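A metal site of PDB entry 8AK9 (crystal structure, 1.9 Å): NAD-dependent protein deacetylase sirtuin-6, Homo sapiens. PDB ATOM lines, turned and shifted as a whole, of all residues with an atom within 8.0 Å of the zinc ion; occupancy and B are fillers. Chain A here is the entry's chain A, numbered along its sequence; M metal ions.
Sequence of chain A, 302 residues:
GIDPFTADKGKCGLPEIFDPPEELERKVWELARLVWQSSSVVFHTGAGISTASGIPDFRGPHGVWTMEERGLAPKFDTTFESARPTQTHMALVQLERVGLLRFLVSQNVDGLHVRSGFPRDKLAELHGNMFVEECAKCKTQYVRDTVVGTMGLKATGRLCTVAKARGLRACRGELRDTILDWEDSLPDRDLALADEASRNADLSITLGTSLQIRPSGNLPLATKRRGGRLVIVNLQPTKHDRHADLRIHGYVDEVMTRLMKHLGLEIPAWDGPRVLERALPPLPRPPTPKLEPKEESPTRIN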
ATOM      1  N   GLU A 134     -11.229  -9.180  -8.547  1.00  0.00           N
ATOM      2  CA  GLU A 134     -11.082  -8.353  -9.764  1.00  0.00           C
ATOM      3  C   GLU A 134     -10.563  -9.232 -10.913  1.00  0.00           C
ATOM      4  O   GLU A 134      -9.616 -10.006 -10.698  1.00  0.00           O
ATOM      5  CB  GLU A 134     -10.158  -7.174  -9.475  1.00  0.00           C
ATOM      6  CG  GLU A 134      -9.910  -6.289 -10.683  1.00  0.00           C
ATOM      7  CD  GLU A 134      -9.001  -5.104 -10.412  1.00  0.00           C
ATOM      8  OE1 GLU A 134      -9.327  -4.298  -9.525  1.00  0.00           O
ATOM      9  OE2 GLU A 134      -7.968  -4.990 -11.094  1.00  0.00           O
ATOM     10  N   CYS A 135     -11.172  -9.127 -12.087  1.00  0.00           N
ATOM     11  CA  CYS A 135     -10.733  -9.882 -13.280  1.00  0.00           C
ATOM     12  C   CYS A 135      -9.404  -9.289 -13.744  1.00  0.00           C
ATOM     13  O   CYS A 135      -9.320  -8.063 -13.942  1.00  0.00           O
ATOM     14  CB  CYS A 135     -11.775  -9.800 -14.394  1.00  0.00           C
ATOM     15  SG  CYS A 135     -11.297 -10.646 -15.933  1.00  0.00           S
ATOM     16  N   ALA A 136      -8.393 -10.141 -13.879  1.00  0.00           N
ATOM     17  CA  ALA A 136      -7.071  -9.733 -14.399  1.00  0.00           C
ATOM     18  C   ALA A 136      -7.249  -9.136 -15.797  1.00  0.00           C
ATOM     19  O   ALA A 136      -6.565  -8.144 -16.113  1.00  0.00           O
ATOM     20  CB  ALA A 136      -6.166 -10.931 -14.405  1.00  0.00           C
ATOM     21  N   LYS A 137      -8.158  -9.691 -16.605  1.00  0.00           N
ATOM     22  CA  LYS A 137      -8.317  -9.283 -18.021  1.00  0.00           C
ATOM     23  C   LYS A 137      -9.137  -7.996 -18.125  1.00  0.00           C
ATOM     24  O   LYS A 137      -8.577  -7.014 -18.639  1.00  0.00           O
ATOM     25  CB  LYS A 137      -9.000 -10.363 -18.853  1.00  0.00           C
ATOM     26  CG  LYS A 137      -8.222 -11.656 -19.008  1.00  0.00           C
ATOM     27  CD  LYS A 137      -8.938 -12.644 -19.895  1.00  0.00           C
ATOM     28  CE  LYS A 137      -8.115 -13.871 -20.217  1.00  0.00           C
ATOM     29  NZ  LYS A 137      -8.871 -14.815 -21.072  1.00  0.00           N
ATOM     30  N   CYS A 138     -10.417  -8.001 -17.711  1.00  0.00           N
ATOM     31  CA  CYS A 138     -11.342  -6.863 -17.985  1.00  0.00           C
ATOM     32  C   CYS A 138     -11.438  -5.924 -16.789  1.00  0.00           C
ATOM     33  O   CYS A 138     -12.131  -4.906 -16.930  1.00  0.00           O
ATOM     34  CB  CYS A 138     -12.722  -7.336 -18.418  1.00  0.00           C
ATOM     35  SG  CYS A 138     -13.669  -8.194 -17.134  1.00  0.00           S
ATOM     36  N   LYS A 139     -10.817  -6.264 -15.655  1.00  0.00           N
ATOM     37  CA  LYS A 139     -10.743  -5.402 -14.441  1.00  0.00           C
ATOM     38  C   LYS A 139     -12.110  -5.342 -13.745  1.00  0.00           C
ATOM     39  O   LYS A 139     -12.243  -4.518 -12.813  1.00  0.00           O
ATOM     40  CB  LYS A 139     -10.188  -4.017 -14.818  1.00  0.00           C
ATOM     41  CG  LYS A 139      -8.841  -4.041 -15.523  1.00  0.00           C
ATOM     42  CD  LYS A 139      -7.742  -4.712 -14.715  1.00  0.00           C
ATOM     43  CE  LYS A 139      -6.413  -4.762 -15.453  1.00  0.00           C
ATOM     44  NZ  LYS A 139      -5.403  -5.556 -14.709  1.00  0.00           N
ATOM     45  N   THR A 140     -13.073  -6.167 -14.145  1.00  0.00           N
ATOM     46  CA  THR A 140     -14.437  -6.183 -13.539  1.00  0.00           C
ATOM     47  C   THR A 140     -14.305  -6.665 -12.083  1.00  0.00           C
ATOM     48  O   THR A 140     -13.765  -7.753 -11.875  1.00  0.00           O
ATOM     49  CB  THR A 140     -15.425  -7.072 -14.297  1.00  0.00           C
ATOM     50  OG1 THR A 140     -15.437  -6.646 -15.658  1.00  0.00           O
ATOM     51  CG2 THR A 140     -16.837  -7.005 -13.721  1.00  0.00           C
ATOM     52  N   GLN A 141     -14.788  -5.887 -11.125  1.00  0.00           N
ATOM     53  CA  GLN A 141     -14.735  -6.237  -9.685  1.00  0.00           C
ATOM     54  C   GLN A 141     -16.016  -6.965  -9.286  1.00  0.00           C
ATOM     55  O   GLN A 141     -17.072  -6.685  -9.862  1.00  0.00           O
ATOM     56  CB  GLN A 141     -14.478  -4.980  -8.854  1.00  0.00           C
ATOM     57  CG  GLN A 141     -13.105  -4.390  -9.147  1.00  0.00           C
ATOM     58  CD  GLN A 141     -12.727  -3.293  -8.189  1.00  0.00           C
ATOM     59  OE1 GLN A 141     -13.569  -2.558  -7.675  1.00  0.00           O
ATOM     60  NE2 GLN A 141     -11.437  -3.174  -7.928  1.00  0.00           N
ATOM     61  N   TYR A 142     -15.905  -7.939  -8.385  1.00  0.00           N
ATOM     62  CA  TYR A 142     -17.077  -8.660  -7.822  1.00  0.00           C
ATOM     63  C   TYR A 142     -17.073  -8.463  -6.309  1.00  0.00           C
ATOM     64  O   TYR A 142     -16.070  -8.805  -5.629  1.00  0.00           O
ATOM     65  CB  TYR A 142     -17.044 -10.127  -8.230  1.00  0.00           C
ATOM     66  CG  TYR A 142     -17.057 -10.376  -9.720  1.00  0.00           C
ATOM     67  CD1 TYR A 142     -15.948 -10.101 -10.501  1.00  0.00           C
ATOM     68  CD2 TYR A 142     -18.180 -10.899 -10.357  1.00  0.00           C
ATOM     69  CE1 TYR A 142     -15.945 -10.314 -11.870  1.00  0.00           C
ATOM     70  CE2 TYR A 142     -18.191 -11.144 -11.710  1.00  0.00           C
ATOM     71  CZ  TYR A 142     -17.075 -10.845 -12.477  1.00  0.00           C
ATOM     72  OH  TYR A 142     -17.062 -11.068 -13.820  1.00  0.00           O
ATOM     73  N   LEU A 159     -13.635 -17.614 -11.960  1.00  0.00           N
ATOM     74  CA  LEU A 159     -13.426 -16.955 -13.283  1.00  0.00           C
ATOM     75  C   LEU A 159     -14.476 -15.859 -13.523  1.00  0.00           C
ATOM     76  O   LEU A 159     -15.588 -15.920 -12.938  1.00  0.00           O
ATOM     77  CB  LEU A 159     -13.501 -17.974 -14.414  1.00  0.00           C
ATOM     78  CG  LEU A 159     -12.409 -19.045 -14.458  1.00  0.00           C
ATOM     79  CD1 LEU A 159     -12.550 -19.876 -15.721  1.00  0.00           C
ATOM     80  CD2 LEU A 159     -11.016 -18.431 -14.363  1.00  0.00           C
ATOM     81  N   CYS A 160     -14.130 -14.918 -14.396  1.00  0.00           N
ATOM     82  CA  CYS A 160     -15.015 -13.808 -14.817  1.00  0.00           C
ATOM     83  C   CYS A 160     -16.261 -14.382 -15.508  1.00  0.00           C
ATOM     84  O   CYS A 160     -16.111 -15.386 -16.211  1.00  0.00           O
ATOM     85  CB  CYS A 160     -14.263 -12.889 -15.759  1.00  0.00           C
ATOM     86  SG  CYS A 160     -15.020 -11.260 -15.859  1.00  0.00           S
ATOM     87  N   THR A 161     -17.423 -13.746 -15.303  1.00  0.00           N
ATOM     88  CA  THR A 161     -18.750 -14.153 -15.862  1.00  0.00           C
ATOM     89  C   THR A 161     -19.286 -13.082 -16.833  1.00  0.00           C
ATOM     90  O   THR A 161     -20.424 -13.255 -17.311  1.00  0.00           O
ATOM     91  CB  THR A 161     -19.762 -14.430 -14.734  1.00  0.00           C
ATOM     92  OG1 THR A 161     -19.939 -13.236 -13.969  1.00  0.00           O
ATOM     93  CG2 THR A 161     -19.331 -15.555 -13.821  1.00  0.00           C
ATOM     94  N   VAL A 162     -18.514 -12.030 -17.123  1.00  0.00           N
ATOM     95  CA  VAL A 162     -18.930 -10.912 -18.017  1.00  0.00           C
ATOM     96  C   VAL A 162     -19.134 -11.472 -19.439  1.00  0.00           C
ATOM     97  O   VAL A 162     -18.228 -12.180 -19.930  1.00  0.00           O
ATOM     98  CB  VAL A 162     -17.913  -9.753 -17.989  1.00  0.00           C
ATOM     99  CG1 VAL A 162     -18.165  -8.721 -19.082  1.00  0.00           C
ATOM    100  CG2 VAL A 162     -17.889  -9.081 -16.625  1.00  0.00           C
ATOM    101  N   ALA A 163     -20.282 -11.131 -20.043  1.00  0.00           N
ATOM    102  CA  ALA A 163     -20.803 -11.636 -21.342  1.00  0.00           C
ATOM    103  C   ALA A 163     -19.703 -11.625 -22.419  1.00  0.00           C
ATOM    104  O   ALA A 163     -19.562 -10.576 -23.084  1.00  0.00           O
ATOM    105  CB  ALA A 163     -21.994 -10.815 -21.763  1.00  0.00           C
ATOM    106  N   CYS A 171     -15.453 -13.808 -21.241  1.00  0.00           N
ATOM    107  CA  CYS A 171     -14.144 -13.377 -20.670  1.00  0.00           C
ATOM    108  C   CYS A 171     -13.452 -14.578 -20.006  1.00  0.00           C
ATOM    109  O   CYS A 171     -12.267 -14.831 -20.335  1.00  0.00           O
ATOM    110  CB  CYS A 171     -14.335 -12.270 -19.644  1.00  0.00           C
ATOM    111  SG  CYS A 171     -12.788 -11.469 -19.164  1.00  0.00           S
ATOM    112  N   ARG A 172     -14.161 -15.270 -19.117  1.00  0.00           N
ATOM    113  CA  ARG A 172     -13.613 -16.393 -18.296  1.00  0.00           C
ATOM    114  C   ARG A 172     -12.240 -15.994 -17.761  1.00  0.00           C
ATOM    115  O   ARG A 172     -11.399 -16.899 -17.527  1.00  0.00           O
ATOM    116  CB  ARG A 172     -13.558 -17.680 -19.131  1.00  0.00           C
ATOM    117  CG  ARG A 172     -14.893 -18.086 -19.732  1.00  0.00           C
ATOM    118  CD  ARG A 172     -15.109 -19.598 -19.775  1.00  0.00           C
ATOM    119  NE  ARG A 172     -13.892 -20.339 -20.090  1.00  0.00           N
ATOM    120  CZ  ARG A 172     -13.286 -21.241 -19.303  1.00  0.00           C
ATOM    121  NH1 ARG A 172     -13.794 -21.554 -18.121  1.00  0.00           N
ATOM    122  NH2 ARG A 172     -12.182 -21.832 -19.719  1.00  0.00           N
ATOM    123  N   GLY A 173     -12.024 -14.696 -17.537  1.00  0.00           N
ATOM    124  CA  GLY A 173     -10.749 -14.152 -17.012  1.00  0.00           C
ATOM    125  C   GLY A 173     -10.458 -14.652 -15.607  1.00  0.00           C
ATOM    126  O   GLY A 173     -11.426 -14.934 -14.858  1.00  0.00           O
ATOM    127  N   GLU A 174      -9.182 -14.763 -15.263  1.00  0.00           N
ATOM    128  CA  GLU A 174      -8.694 -15.184 -13.920  1.00  0.00           C
ATOM    129  C   GLU A 174      -9.123 -14.133 -12.894  1.00  0.00           C
ATOM    130  O   GLU A 174      -8.746 -12.950 -13.063  1.00  0.00           O
ATOM    131  CB  GLU A 174      -7.166 -15.378 -13.968  1.00  0.00           C
ATOM    132  CG  GLU A 174      -6.573 -15.994 -12.706  1.00  0.00           C
ATOM    133  CD  GLU A 174      -5.131 -16.453 -12.837  1.00  0.00           C
ATOM    134  OE1 GLU A 174      -4.806 -17.155 -13.830  1.00  0.00           O
ATOM    135  OE2 GLU A 174      -4.316 -16.110 -11.949  1.00  0.00           O
ATOM    136  N   LEU A 175      -9.915 -14.533 -11.898  1.00  0.00           N
ATOM    137  CA  LEU A 175     -10.326 -13.667 -10.765  1.00  0.00           C
ATOM    138  C   LEU A 175      -9.231 -13.683  -9.704  1.00  0.00           C
ATOM    139  O   LEU A 175      -8.772 -14.798  -9.333  1.00  0.00           O
ATOM    140  CB  LEU A 175     -11.661 -14.113 -10.171  1.00  0.00           C
ATOM    141  CG  LEU A 175     -12.903 -13.795 -11.009  1.00  0.00           C
ATOM    142  CD1 LEU A 175     -14.169 -13.920 -10.160  1.00  0.00           C
ATOM    143  CD2 LEU A 175     -12.806 -12.424 -11.654  1.00  0.00           C
HETATM  144 ZN    ZN M   1     -13.229 -10.403 -17.062  1.00  0.00          ZN
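The backbone NH (N) of Cys 135 is in hydrogen-bond range of the backbone carbonyl oxygen (O) of Thr 140, at 2.9 Å. The side-chain sulfur (SG) of Cys 135 sits close to the backbone NH (N) of Lys 137, at 3.3 Å. The side-chain hydroxyl (OG1) of Thr 140 lies close to the side-chain sulfur (SG) of Cys 138 (2.8 Å). The backbone NH of Cys 160 is in hydrogen-bond range of the backbone carbonyl oxygen of Gly 173 (2.7 Å). The backbone NH (N) of Val 162 sits close to the side-chain sulfur (SG) of Cys 160 (3.8 Å). SG of Cys 160 lies close to OH of Tyr 142, at 2.9 Å. O of Cys 171 is in hydrogen-bond range of NZ of Lys 137, at 3.5 Å. The backbone NH (N) of Cys 171 sits at hydrogen-bond distance from the backbone carbonyl oxygen (O) of Val 162, at 3.5 Å.
Four residues have an atom within 4 Å of the zinc ion: Cys 135, Cys 138, Cys 160 and Cys 171.
The zinc ion is bound by SG of Cys 135 (2.3 Å), SG of Cys 138 (2.3 Å), SG of Cys 160 (2.3 Å) and SG of Cys 171 (2.4 Å). The zinc ion has four donor atoms within binding distance.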
